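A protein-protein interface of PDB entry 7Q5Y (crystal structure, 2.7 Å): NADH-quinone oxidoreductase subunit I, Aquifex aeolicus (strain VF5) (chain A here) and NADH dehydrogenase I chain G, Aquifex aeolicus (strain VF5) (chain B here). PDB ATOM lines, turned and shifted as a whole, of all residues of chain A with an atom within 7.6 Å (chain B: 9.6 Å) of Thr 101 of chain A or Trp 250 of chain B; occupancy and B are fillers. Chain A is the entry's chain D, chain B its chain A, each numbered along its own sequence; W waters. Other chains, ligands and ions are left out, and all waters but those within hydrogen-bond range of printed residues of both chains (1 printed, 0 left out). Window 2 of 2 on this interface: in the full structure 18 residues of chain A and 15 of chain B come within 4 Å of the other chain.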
ATOM      1  N   TYR A  91     -33.012  -3.832  -3.399  1.00  0.00           N
ATOM      2  CA  TYR A  91     -31.812  -4.141  -4.172  1.00  0.00           C
ATOM      3  C   TYR A  91     -32.109  -4.753  -5.535  1.00  0.00           C
ATOM      4  O   TYR A  91     -31.206  -5.308  -6.159  1.00  0.00           O
ATOM      5  CB  TYR A  91     -30.848  -5.039  -3.390  1.00  0.00           C
ATOM      6  CG  TYR A  91     -30.170  -4.352  -2.223  1.00  0.00           C
ATOM      7  CD1 TYR A  91     -30.808  -4.238  -0.990  1.00  0.00           C
ATOM      8  CD2 TYR A  91     -28.886  -3.825  -2.348  1.00  0.00           C
ATOM      9  CE1 TYR A  91     -30.195  -3.615   0.076  1.00  0.00           C
ATOM     10  CE2 TYR A  91     -28.256  -3.194  -1.285  1.00  0.00           C
ATOM     11  CZ  TYR A  91     -28.914  -3.096  -0.072  1.00  0.00           C
ATOM     12  OH  TYR A  91     -28.291  -2.485   0.997  1.00  0.00           O
ATOM     13  N   GLN A  94     -30.252  -2.490  -8.415  1.00  0.00           N
ATOM     14  CA  GLN A  94     -28.827  -2.792  -8.455  1.00  0.00           C
ATOM     15  C   GLN A  94     -28.551  -4.226  -8.881  1.00  0.00           C
ATOM     16  O   GLN A  94     -27.549  -4.488  -9.555  1.00  0.00           O
ATOM     17  CB  GLN A  94     -28.197  -2.537  -7.092  1.00  0.00           C
ATOM     18  CG  GLN A  94     -26.684  -2.704  -7.071  1.00  0.00           C
ATOM     19  CD  GLN A  94     -26.151  -2.283  -5.750  1.00  0.00           C
ATOM     20  OE1 GLN A  94     -26.863  -2.355  -4.768  1.00  0.00           O
ATOM     21  NE2 GLN A  94     -24.907  -1.833  -5.703  1.00  0.00           N
ATOM     22  N   THR A  95     -29.407  -5.172  -8.482  1.00  0.00           N
ATOM     23  CA  THR A  95     -29.170  -6.560  -8.869  1.00  0.00           C
ATOM     24  C   THR A  95     -29.435  -6.766 -10.344  1.00  0.00           C
ATOM     25  O   THR A  95     -28.720  -7.532 -10.994  1.00  0.00           O
ATOM     26  CB  THR A  95     -30.033  -7.517  -8.052  1.00  0.00           C
ATOM     27  OG1 THR A  95     -29.837  -7.256  -6.659  1.00  0.00           O
ATOM     28  CG2 THR A  95     -29.674  -8.972  -8.357  1.00  0.00           C
ATOM     29  N   ALA A  96     -30.427  -6.059 -10.895  1.00  0.00           N
ATOM     30  CA  ALA A  96     -30.760  -6.178 -12.317  1.00  0.00           C
ATOM     31  C   ALA A  96     -29.753  -5.451 -13.197  1.00  0.00           C
ATOM     32  O   ALA A  96     -29.492  -5.881 -14.331  1.00  0.00           O
ATOM     33  CB  ALA A  96     -32.162  -5.622 -12.565  1.00  0.00           C
ATOM     34  N   CYS A  97     -29.194  -4.361 -12.672  1.00  0.00           N
ATOM     35  CA  CYS A  97     -28.209  -3.548 -13.358  1.00  0.00           C
ATOM     36  C   CYS A  97     -26.959  -4.340 -13.737  1.00  0.00           C
ATOM     37  O   CYS A  97     -26.396  -5.040 -12.878  1.00  0.00           O
ATOM     38  CB  CYS A  97     -27.817  -2.412 -12.416  1.00  0.00           C
ATOM     39  SG  CYS A  97     -26.535  -1.329 -13.013  1.00  0.00           S
ATOM     40  N   PRO A  98     -26.452  -4.204 -14.975  1.00  0.00           N
ATOM     41  CA  PRO A  98     -25.219  -4.919 -15.342  1.00  0.00           C
ATOM     42  C   PRO A  98     -23.992  -4.295 -14.711  1.00  0.00           C
ATOM     43  O   PRO A  98     -22.934  -4.936 -14.677  1.00  0.00           O
ATOM     44  CB  PRO A  98     -25.162  -4.794 -16.874  1.00  0.00           C
ATOM     45  CG  PRO A  98     -26.498  -4.247 -17.287  1.00  0.00           C
ATOM     46  CD  PRO A  98     -27.000  -3.457 -16.118  1.00  0.00           C
ATOM     47  N   MET A  99     -24.116  -3.065 -14.212  1.00  0.00           N
ATOM     48  CA  MET A  99     -23.038  -2.323 -13.560  1.00  0.00           C
ATOM     49  C   MET A  99     -23.393  -2.001 -12.107  1.00  0.00           C
ATOM     50  O   MET A  99     -23.410  -0.827 -11.707  1.00  0.00           O
ATOM     51  CB  MET A  99     -22.774  -1.044 -14.348  1.00  0.00           C
ATOM     52  CG  MET A  99     -22.214  -1.311 -15.727  1.00  0.00           C
ATOM     53  SD  MET A  99     -20.481  -1.812 -15.595  1.00  0.00           S
ATOM     54  CE  MET A  99     -19.829  -0.391 -14.709  1.00  0.00           C
ATOM     55  N   PRO A 100     -23.682  -3.017 -11.286  1.00  0.00           N
ATOM     56  CA  PRO A 100     -24.072  -2.737  -9.895  1.00  0.00           C
ATOM     57  C   PRO A 100     -23.107  -1.860  -9.110  1.00  0.00           C
ATOM     58  O   PRO A 100     -23.539  -1.191  -8.160  1.00  0.00           O
ATOM     59  CB  PRO A 100     -24.199  -4.140  -9.281  1.00  0.00           C
ATOM     60  CG  PRO A 100     -23.334  -5.015 -10.126  1.00  0.00           C
ATOM     61  CD  PRO A 100     -23.463  -4.461 -11.510  1.00  0.00           C
ATOM     62  N   THR A 101     -21.824  -1.835  -9.456  1.00  0.00           N
ATOM     63  CA  THR A 101     -20.909  -1.009  -8.672  1.00  0.00           C
ATOM     64  C   THR A 101     -21.323   0.457  -8.652  1.00  0.00           C
ATOM     65  O   THR A 101     -21.012   1.160  -7.692  1.00  0.00           O
ATOM     66  CB  THR A 101     -19.476  -1.140  -9.184  1.00  0.00           C
ATOM     67  OG1 THR A 101     -19.403  -0.810 -10.587  1.00  0.00           O
ATOM     68  CG2 THR A 101     -19.004  -2.542  -8.960  1.00  0.00           C
ATOM     69  N   LEU A 102     -22.018   0.945  -9.682  1.00  0.00           N
ATOM     70  CA  LEU A 102     -22.396   2.354  -9.682  1.00  0.00           C
ATOM     71  C   LEU A 102     -23.421   2.697  -8.603  1.00  0.00           C
ATOM     72  O   LEU A 102     -23.553   3.877  -8.248  1.00  0.00           O
ATOM     73  CB  LEU A 102     -22.895   2.772 -11.070  1.00  0.00           C
ATOM     74  CG  LEU A 102     -24.272   2.380 -11.594  1.00  0.00           C
ATOM     75  CD1 LEU A 102     -25.307   3.432 -11.192  1.00  0.00           C
ATOM     76  CD2 LEU A 102     -24.189   2.254 -13.096  1.00  0.00           C
ATOM     77  N   PHE A 103     -24.147   1.713  -8.076  1.00  0.00           N
ATOM     78  CA  PHE A 103     -25.136   1.955  -7.029  1.00  0.00           C
ATOM     79  C   PHE A 103     -24.509   1.852  -5.640  1.00  0.00           C
ATOM     80  O   PHE A 103     -23.446   1.257  -5.455  1.00  0.00           O
ATOM     81  CB  PHE A 103     -26.262   0.915  -7.071  1.00  0.00           C
ATOM     82  CG  PHE A 103     -27.360   1.190  -8.054  1.00  0.00           C
ATOM     83  CD1 PHE A 103     -28.459   1.958  -7.684  1.00  0.00           C
ATOM     84  CD2 PHE A 103     -27.345   0.606  -9.310  1.00  0.00           C
ATOM     85  CE1 PHE A 103     -29.500   2.180  -8.561  1.00  0.00           C
ATOM     86  CE2 PHE A 103     -28.376   0.820 -10.196  1.00  0.00           C
ATOM     87  CZ  PHE A 103     -29.456   1.611  -9.824  1.00  0.00           C
ATOM     88  N   ARG A 104     -25.213   2.411  -4.649  1.00  0.00           N
ATOM     89  CA  ARG A 104     -24.824   2.279  -3.241  1.00  0.00           C
ATOM     90  C   ARG A 104     -26.108   2.494  -2.439  1.00  0.00           C
ATOM     91  O   ARG A 104     -26.567   3.636  -2.298  1.00  0.00           O
ATOM     92  CB  ARG A 104     -23.728   3.226  -2.821  1.00  0.00           C
ATOM     93  CG  ARG A 104     -22.613   2.483  -2.091  1.00  0.00           C
ATOM     94  CD  ARG A 104     -22.001   1.536  -3.097  1.00  0.00           C
ATOM     95  NE  ARG A 104     -20.720   0.960  -2.735  1.00  0.00           N
ATOM     96  CZ  ARG A 104     -19.798   0.628  -3.639  1.00  0.00           C
ATOM     97  NH1 ARG A 104     -20.023   0.835  -4.936  1.00  0.00           N
ATOM     98  NH2 ARG A 104     -18.635   0.122  -3.247  1.00  0.00           N
ATOM     99  N   ILE A 105     -26.685   1.387  -1.951  1.00  0.00           N
ATOM    100  CA  ILE A 105     -27.938   1.385  -1.198  1.00  0.00           C
ATOM    101  C   ILE A 105     -27.692   0.861   0.212  1.00  0.00           C
ATOM    102  O   ILE A 105     -26.966  -0.120   0.397  1.00  0.00           O
ATOM    103  CB  ILE A 105     -29.006   0.521  -1.902  1.00  0.00           C
ATOM    104  CG1 ILE A 105     -29.158   0.926  -3.370  1.00  0.00           C
ATOM    105  CG2 ILE A 105     -30.315   0.631  -1.179  1.00  0.00           C
ATOM    106  CD1 ILE A 105     -29.877  -0.117  -4.241  1.00  0.00           C
ATOM    107  N   GLU A 106     -28.307   1.501   1.204  1.00  0.00           N
ATOM    108  CA  GLU A 106     -28.167   1.083   2.594  1.00  0.00           C
ATOM    109  C   GLU A 106     -29.493   1.304   3.306  1.00  0.00           C
ATOM    110  O   GLU A 106     -30.131   2.352   3.144  1.00  0.00           O
ATOM    111  CB  GLU A 106     -27.065   1.854   3.346  1.00  0.00           C
ATOM    112  CG  GLU A 106     -25.626   1.455   3.033  1.00  0.00           C
ATOM    113  CD  GLU A 106     -24.594   2.353   3.740  1.00  0.00           C
ATOM    114  OE1 GLU A 106     -24.917   2.899   4.824  1.00  0.00           O
ATOM    115  OE2 GLU A 106     -23.471   2.535   3.201  1.00  0.00           O
ATOM    116  N   ASP A 121     -27.198   6.097  -3.490  1.00  0.00           N
ATOM    117  CA  ASP A 121     -26.360   6.880  -4.389  1.00  0.00           C
ATOM    118  C   ASP A 121     -26.143   6.150  -5.712  1.00  0.00           C
ATOM    119  O   ASP A 121     -26.034   4.922  -5.745  1.00  0.00           O
ATOM    120  CB  ASP A 121     -24.967   7.195  -3.764  1.00  0.00           C
ATOM    121  CG  ASP A 121     -25.046   7.860  -2.386  1.00  0.00           C
ATOM    122  OD1 ASP A 121     -26.079   8.495  -2.076  1.00  0.00           O
ATOM    123  OD2 ASP A 121     -24.034   7.800  -1.639  1.00  0.00           O
ATOM    124  N   MET A 122     -26.071   6.922  -6.799  1.00  0.00           N
ATOM    125  CA  MET A 122     -25.842   6.419  -8.146  1.00  0.00           C
ATOM    126  C   MET A 122     -24.796   7.278  -8.846  1.00  0.00           C
ATOM    127  O   MET A 122     -24.858   8.513  -8.801  1.00  0.00           O
ATOM    128  CB  MET A 122     -27.118   6.423  -8.998  1.00  0.00           C
ATOM    129  CG  MET A 122     -28.312   5.725  -8.386  1.00  0.00           C
ATOM    130  SD  MET A 122     -29.677   5.684  -9.544  1.00  0.00           S
ATOM    131  CE  MET A 122     -28.855   4.802 -10.854  1.00  0.00           C
ATOM    132  N   ASN A 123     -23.854   6.618  -9.515  1.00  0.00           N
ATOM    133  CA  ASN A 123     -22.791   7.287 -10.261  1.00  0.00           C
ATOM    134  C   ASN A 123     -23.159   7.155 -11.735  1.00  0.00           C
ATOM    135  O   ASN A 123     -22.940   6.104 -12.343  1.00  0.00           O
ATOM    136  CB  ASN A 123     -21.428   6.674  -9.946  1.00  0.00           C
ATOM    137  CG  ASN A 123     -20.359   7.092 -10.936  1.00  0.00           C
ATOM    138  OD1 ASN A 123     -19.629   6.248 -11.448  1.00  0.00           O
ATOM    139  ND2 ASN A 123     -20.274   8.391 -11.230  1.00  0.00           N
ATOM    140  N   ASN A 126     -21.001   5.744 -15.089  1.00  0.00           N
ATOM    141  CA  ASN A 126     -20.733   4.342 -15.398  1.00  0.00           C
ATOM    142  C   ASN A 126     -22.022   3.637 -15.770  1.00  0.00           C
ATOM    143  O   ASN A 126     -22.076   2.406 -15.804  1.00  0.00           O
ATOM    144  CB  ASN A 126     -20.065   3.645 -14.214  1.00  0.00           C
ATOM    145  CG  ASN A 126     -18.599   3.957 -14.127  1.00  0.00           C
ATOM    146  OD1 ASN A 126     -17.804   3.502 -14.948  1.00  0.00           O
ATOM    147  ND2 ASN A 126     -18.230   4.777 -13.151  1.00  0.00           N
ATOM    148  N   TRP B 219     -31.776  -6.025   7.420  1.00  0.00           N
ATOM    149  CA  TRP B 219     -30.386  -5.582   7.366  1.00  0.00           C
ATOM    150  C   TRP B 219     -29.728  -5.861   6.024  1.00  0.00           C
ATOM    151  O   TRP B 219     -28.778  -5.163   5.656  1.00  0.00           O
ATOM    152  CB  TRP B 219     -29.574  -6.237   8.486  1.00  0.00           C
ATOM    153  CG  TRP B 219     -29.981  -5.760   9.824  1.00  0.00           C
ATOM    154  CD1 TRP B 219     -30.656  -6.462  10.790  1.00  0.00           C
ATOM    155  CD2 TRP B 219     -29.781  -4.447  10.349  1.00  0.00           C
ATOM    156  NE1 TRP B 219     -30.859  -5.665  11.899  1.00  0.00           N
ATOM    157  CE2 TRP B 219     -30.340  -4.422  11.647  1.00  0.00           C
ATOM    158  CE3 TRP B 219     -29.179  -3.291   9.855  1.00  0.00           C
ATOM    159  CZ2 TRP B 219     -30.308  -3.283  12.450  1.00  0.00           C
ATOM    160  CZ3 TRP B 219     -29.143  -2.162  10.667  1.00  0.00           C
ATOM    161  CH2 TRP B 219     -29.700  -2.171  11.949  1.00  0.00           C
ATOM    162  N   SER B 220     -30.207  -6.850   5.279  1.00  0.00           N
ATOM    163  CA  SER B 220     -29.575  -7.165   4.006  1.00  0.00           C
ATOM    164  C   SER B 220     -30.578  -7.925   3.139  1.00  0.00           C
ATOM    165  O   SER B 220     -31.789  -7.870   3.375  1.00  0.00           O
ATOM    166  CB  SER B 220     -28.280  -7.954   4.272  1.00  0.00           C
ATOM    167  OG  SER B 220     -27.488  -8.083   3.109  1.00  0.00           O
ATOM    168  N   ARG B 221     -30.072  -8.606   2.121  1.00  0.00           N
ATOM    169  CA  ARG B 221     -30.830  -9.453   1.219  1.00  0.00           C
ATOM    170  C   ARG B 221     -30.033 -10.746   1.135  1.00  0.00           C
ATOM    171  O   ARG B 221     -28.798 -10.724   1.129  1.00  0.00           O
ATOM    172  CB  ARG B 221     -31.034  -8.855  -0.180  1.00  0.00           C
ATOM    173  CG  ARG B 221     -31.579  -7.455  -0.157  1.00  0.00           C
ATOM    174  CD  ARG B 221     -32.998  -7.453   0.355  1.00  0.00           C
ATOM    175  NE  ARG B 221     -33.982  -7.640  -0.691  1.00  0.00           N
ATOM    176  CZ  ARG B 221     -35.188  -8.138  -0.463  1.00  0.00           C
ATOM    177  NH1 ARG B 221     -35.499  -8.509   0.764  1.00  0.00           N
ATOM    178  NH2 ARG B 221     -36.061  -8.286  -1.457  1.00  0.00           N
ATOM    179  N   TRP B 223     -29.277 -12.793  -1.186  1.00  0.00           N
ATOM    180  CA  TRP B 223     -28.302 -12.974  -2.262  1.00  0.00           C
ATOM    181  C   TRP B 223     -27.111 -12.024  -2.185  1.00  0.00           C
ATOM    182  O   TRP B 223     -26.222 -12.096  -3.038  1.00  0.00           O
ATOM    183  CB  TRP B 223     -28.999 -12.864  -3.633  1.00  0.00           C
ATOM    184  CG  TRP B 223     -29.531 -11.513  -3.986  1.00  0.00           C
ATOM    185  CD1 TRP B 223     -28.887 -10.528  -4.699  1.00  0.00           C
ATOM    186  CD2 TRP B 223     -30.819 -10.991  -3.659  1.00  0.00           C
ATOM    187  NE1 TRP B 223     -29.703  -9.433  -4.835  1.00  0.00           N
ATOM    188  CE2 TRP B 223     -30.895  -9.688  -4.202  1.00  0.00           C
ATOM    189  CE3 TRP B 223     -31.916 -11.489  -2.949  1.00  0.00           C
ATOM    190  CZ2 TRP B 223     -32.028  -8.883  -4.060  1.00  0.00           C
ATOM    191  CZ3 TRP B 223     -33.040 -10.690  -2.815  1.00  0.00           C
ATOM    192  CH2 TRP B 223     -33.086  -9.398  -3.370  1.00  0.00           C
ATOM    193  N   LEU B 224     -27.055 -11.148  -1.192  1.00  0.00           N
ATOM    194  CA  LEU B 224     -25.946 -10.218  -1.057  1.00  0.00           C
ATOM    195  C   LEU B 224     -24.898 -10.682  -0.056  1.00  0.00           C
ATOM    196  O   LEU B 224     -23.950  -9.938   0.214  1.00  0.00           O
ATOM    197  CB  LEU B 224     -26.469  -8.839  -0.648  1.00  0.00           C
ATOM    198  CG  LEU B 224     -27.436  -8.194  -1.626  1.00  0.00           C
ATOM    199  CD1 LEU B 224     -28.012  -6.920  -1.053  1.00  0.00           C
ATOM    200  CD2 LEU B 224     -26.715  -7.926  -2.894  1.00  0.00           C
ATOM    201  N   LEU B 225     -25.033 -11.884   0.495  1.00  0.00           N
ATOM    202  CA  LEU B 225     -24.100 -12.382   1.490  1.00  0.00           C
ATOM    203  C   LEU B 225     -23.218 -13.511   0.964  1.00  0.00           C
ATOM    204  O   LEU B 225     -23.541 -14.198  -0.006  1.00  0.00           O
ATOM    205  CB  LEU B 225     -24.868 -12.874   2.722  1.00  0.00           C
ATOM    206  CG  LEU B 225     -25.823 -11.865   3.359  1.00  0.00           C
ATOM    207  CD1 LEU B 225     -26.612 -12.436   4.530  1.00  0.00           C
ATOM    208  CD2 LEU B 225     -25.005 -10.671   3.780  1.00  0.00           C
ATOM    209  N   GLY B 246     -20.648 -10.577   5.096  1.00  0.00           N
ATOM    210  CA  GLY B 246     -20.385  -9.570   4.095  1.00  0.00           C
ATOM    211  C   GLY B 246     -18.891  -9.261   4.091  1.00  0.00           C
ATOM    212  O   GLY B 246     -18.136  -9.653   4.975  1.00  0.00           O
ATOM    213  N   VAL B 247     -18.470  -8.525   3.076  1.00  0.00           N
ATOM    214  CA  VAL B 247     -17.058  -8.217   2.919  1.00  0.00           C
ATOM    215  C   VAL B 247     -16.743  -6.737   2.973  1.00  0.00           C
ATOM    216  O   VAL B 247     -15.602  -6.371   3.297  1.00  0.00           O
ATOM    217  CB  VAL B 247     -16.539  -8.846   1.613  1.00  0.00           C
ATOM    218  CG1 VAL B 247     -15.397  -8.091   1.028  1.00  0.00           C
ATOM    219  CG2 VAL B 247     -16.148 -10.297   1.922  1.00  0.00           C
ATOM    220  N   GLY B 248     -17.687  -5.863   2.697  1.00  0.00           N
ATOM    221  CA  GLY B 248     -17.354  -4.460   2.753  1.00  0.00           C
ATOM    222  C   GLY B 248     -17.462  -3.823   1.390  1.00  0.00           C
ATOM    223  O   GLY B 248     -17.071  -2.664   1.217  1.00  0.00           O
ATOM    224  N   ASP B 249     -17.970  -4.585   0.412  1.00  0.00           N
ATOM    225  CA  ASP B 249     -18.163  -4.125  -0.957  1.00  0.00           C
ATOM    226  C   ASP B 249     -19.575  -3.550  -1.095  1.00  0.00           C
ATOM    227  O   ASP B 249     -20.237  -3.266  -0.092  1.00  0.00           O
ATOM    228  CB  ASP B 249     -17.896  -5.252  -1.960  1.00  0.00           C
ATOM    229  CG  ASP B 249     -18.818  -6.435  -1.786  1.00  0.00           C
ATOM    230  OD1 ASP B 249     -19.806  -6.364  -1.019  1.00  0.00           O
ATOM    231  OD2 ASP B 249     -18.541  -7.453  -2.446  1.00  0.00           O
ATOM    232  N   TRP B 250     -20.050  -3.362  -2.333  1.00  0.00           N
ATOM    233  CA  TRP B 250     -21.377  -2.798  -2.536  1.00  0.00           C
ATOM    234  C   TRP B 250     -22.495  -3.691  -2.018  1.00  0.00           C
ATOM    235  O   TRP B 250     -23.591  -3.190  -1.727  1.00  0.00           O
ATOM    236  CB  TRP B 250     -21.653  -2.534  -4.014  1.00  0.00           C
ATOM    237  CG  TRP B 250     -21.661  -3.732  -4.951  1.00  0.00           C
ATOM    238  CD1 TRP B 250     -20.618  -4.193  -5.706  1.00  0.00           C
ATOM    239  CD2 TRP B 250     -22.777  -4.598  -5.243  1.00  0.00           C
ATOM    240  NE1 TRP B 250     -21.012  -5.286  -6.447  1.00  0.00           N
ATOM    241  CE2 TRP B 250     -22.331  -5.554  -6.184  1.00  0.00           C
ATOM    242  CE3 TRP B 250     -24.110  -4.656  -4.802  1.00  0.00           C
ATOM    243  CZ2 TRP B 250     -23.175  -6.559  -6.698  1.00  0.00           C
ATOM    244  CZ3 TRP B 250     -24.954  -5.668  -5.305  1.00  0.00           C
ATOM    245  CH2 TRP B 250     -24.476  -6.609  -6.235  1.00  0.00           C
ATOM    246  N   ARG B 251     -22.261  -5.000  -1.914  1.00  0.00           N
ATOM    247  CA  ARG B 251     -23.327  -5.894  -1.495  1.00  0.00           C
ATOM    248  C   ARG B 251     -23.626  -5.827  -0.002  1.00  0.00           C
ATOM    249  O   ARG B 251     -24.801  -5.800   0.394  1.00  0.00           O
ATOM    250  CB  ARG B 251     -22.991  -7.336  -1.867  1.00  0.00           C
ATOM    251  CG  ARG B 251     -22.685  -7.626  -3.311  1.00  0.00           C
ATOM    252  CD  ARG B 251     -21.419  -8.444  -3.406  1.00  0.00           C
ATOM    253  NE  ARG B 251     -21.611  -9.833  -3.009  1.00  0.00           N
ATOM    254  CZ  ARG B 251     -20.658 -10.596  -2.463  1.00  0.00           C
ATOM    255  NH1 ARG B 251     -19.445 -10.106  -2.221  1.00  0.00           N
ATOM    256  NH2 ARG B 251     -20.920 -11.857  -2.144  1.00  0.00           N
ATOM    257  N   SER B 252     -22.599  -5.848   0.851  1.00  0.00           N
ATOM    258  CA  SER B 252     -22.890  -5.899   2.282  1.00  0.00           C
ATOM    259  C   SER B 252     -21.674  -5.540   3.120  1.00  0.00           C
ATOM    260  O   SER B 252     -20.525  -5.613   2.663  1.00  0.00           O
ATOM    261  CB  SER B 252     -23.358  -7.304   2.684  1.00  0.00           C
ATOM    262  OG  SER B 252     -22.582  -8.279   1.991  1.00  0.00           O
ATOM    263  N   LYS B 253     -21.954  -5.162   4.371  1.00  0.00           N
ATOM    264  CA  LYS B 253     -20.908  -4.749   5.296  1.00  0.00           C
ATOM    265  C   LYS B 253     -19.991  -5.900   5.661  1.00  0.00           C
ATOM    266  O   LYS B 253     -20.348  -7.074   5.577  1.00  0.00           O
ATOM    267  CB  LYS B 253     -21.509  -4.108   6.549  1.00  0.00           C
ATOM    268  CG  LYS B 253     -22.351  -2.878   6.207  1.00  0.00           C
ATOM    269  CD  LYS B 253     -22.615  -1.924   7.364  1.00  0.00           C
ATOM    270  CE  LYS B 253     -23.514  -0.763   6.912  1.00  0.00           C
ATOM    271  NZ  LYS B 253     -23.284   0.511   7.620  1.00  0.00           N
ATOM    272  N   ARG B 254     -18.774  -5.531   6.059  1.00  0.00           N
ATOM    273  CA  ARG B 254     -17.742  -6.482   6.469  1.00  0.00           C
ATOM    274  C   ARG B 254     -18.052  -6.973   7.884  1.00  0.00           C
ATOM    275  O   ARG B 254     -17.517  -6.485   8.877  1.00  0.00           O
ATOM    276  CB  ARG B 254     -16.373  -5.823   6.374  1.00  0.00           C
ATOM    277  CG  ARG B 254     -15.170  -6.746   6.440  1.00  0.00           C
ATOM    278  CD  ARG B 254     -13.962  -5.969   5.942  1.00  0.00           C
ATOM    279  NE  ARG B 254     -12.673  -6.662   6.004  1.00  0.00           N
ATOM    280  CZ  ARG B 254     -12.152  -7.400   5.029  1.00  0.00           C
ATOM    281  NH1 ARG B 254     -12.813  -7.590   3.895  1.00  0.00           N
ATOM    282  NH2 ARG B 254     -10.953  -7.945   5.190  1.00  0.00           N
ATOM    283  N   TYR B 257     -23.532 -11.613   9.328  1.00  0.00           N
ATOM    284  CA  TYR B 257     -24.921 -11.157   9.393  1.00  0.00           C
ATOM    285  C   TYR B 257     -25.868 -12.144  10.055  1.00  0.00           C
ATOM    286  O   TYR B 257     -26.831 -11.728  10.712  1.00  0.00           O
ATOM    287  CB  TYR B 257     -25.450 -10.827   7.991  1.00  0.00           C
ATOM    288  CG  TYR B 257     -25.105  -9.450   7.459  1.00  0.00           C
ATOM    289  CD1 TYR B 257     -23.861  -9.187   6.889  1.00  0.00           C
ATOM    290  CD2 TYR B 257     -26.028  -8.412   7.511  1.00  0.00           C
ATOM    291  CE1 TYR B 257     -23.538  -7.914   6.391  1.00  0.00           C
ATOM    292  CE2 TYR B 257     -25.709  -7.145   7.021  1.00  0.00           C
ATOM    293  CZ  TYR B 257     -24.462  -6.906   6.461  1.00  0.00           C
ATOM    294  OH  TYR B 257     -24.147  -5.660   5.949  1.00  0.00           O
HETATM  295  O   HOH W   1     -25.233  -1.175  -2.543  1.00  0.00           O
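Of the 16 printed residues of chain B, 4 touch a printed residue of chain A.
Hydrophobic or aromatic side chains of chain A that line the printed part of chain B: Tyr 91 and Pro 100.
O of Leu 224 of chain B is in hydrogen-bond range of OG of Ser 252 of chain B (2.8 Å).
The backbone carbonyl oxygen of Tyr 91 of chain A sits at hydrogen-bond distance from the side-chain hydroxyl of Thr 95 of chain A, 2.4 Å away.
The side-chain hydroxyl (OH) of Tyr 91 of chain A is in hydrogen-bond range of the backbone carbonyl oxygen (O) of Ile 105 of chain A.
NE2 of Gln 94 of chain A sits at hydrogen-bond distance from O of Pro 100 of chain A, 2.9 Å away.
The side-chain amide nitrogen (NE2) of Gln 94 of chain A lies close to the backbone carbonyl oxygen (O) of Phe 103 of chain A.
The backbone carbonyl oxygen (O) of Thr 101 of chain A sits at hydrogen-bond distance from the guanidinium group (NH1) of Arg 104 of chain A (2.9 Å).
Among the printed residues, pairs that only touch across the chains: Tyr 91 of chain A with Arg 221 of chain B (3.4 Å), Tyr 91 of chain A with Leu 224 of chain B (3.5 Å), Gln 94 of chain A with Trp 250 of chain B (3.1 Å), Pro 100 of chain A with Trp 250 of chain B (3.7 Å), Thr 101 of chain A with Trp 250 of chain B (3.99 Å) and Arg 104 of chain A with Trp 250 of chain B (3.7 Å).
The indole nitrogen (NE1) of Trp 223 of chain B sits at hydrogen-bond distance from the side-chain hydroxyl (OG1) of Thr 95 of chain A, 2.8 Å away.
Water W1 lies within hydrogen-bond range of O of Trp 250 of chain B (2.7 Å), OE1 of Gln 94 of chain A (3.0 Å) and N of Ile 105 of chain A (3.0 Å).
Printed residues of chain B within 4 Å of Tyr 91 of chain A: Arg 221 (3.4 Å) and Leu 224 (3.5 Å).
Cys 97 of chain A touches none of the printed residues of chain B.
Pro 100 of chain A touches one residue of chain B.
Of the printed residues of chain B, Thr 101 of chain A touches Trp 250.
Printed residues of chain B within 4 Å of Arg 104 of chain A: Trp 250.
Ile 105 of chain A touches none of the printed residues of chain B.
Of the printed residues of chain A, Arg 221 of chain B touches Tyr 91.
Printed residues of chain A within 4 Å of Trp 223 of chain B: Thr 95.
Of the printed residues of chain A, Leu 224 of chain B touches Tyr 91 (3.5 Å).
Of the printed residues of chain A, Trp 250 of chain B touches Gln 94 (3.1 Å), Pro 100 (3.7 Å), Thr 101 (3.99 Å) and Arg 104 (3.7 Å).
The nearest printed residue of chain A that does not touch Trp 250 of chain B is Phe 103 of chain A (4.4 Å).
The nearest printed residue of chain B that does not touch Thr 95 of chain A is Leu 224 of chain B (4.9 Å).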
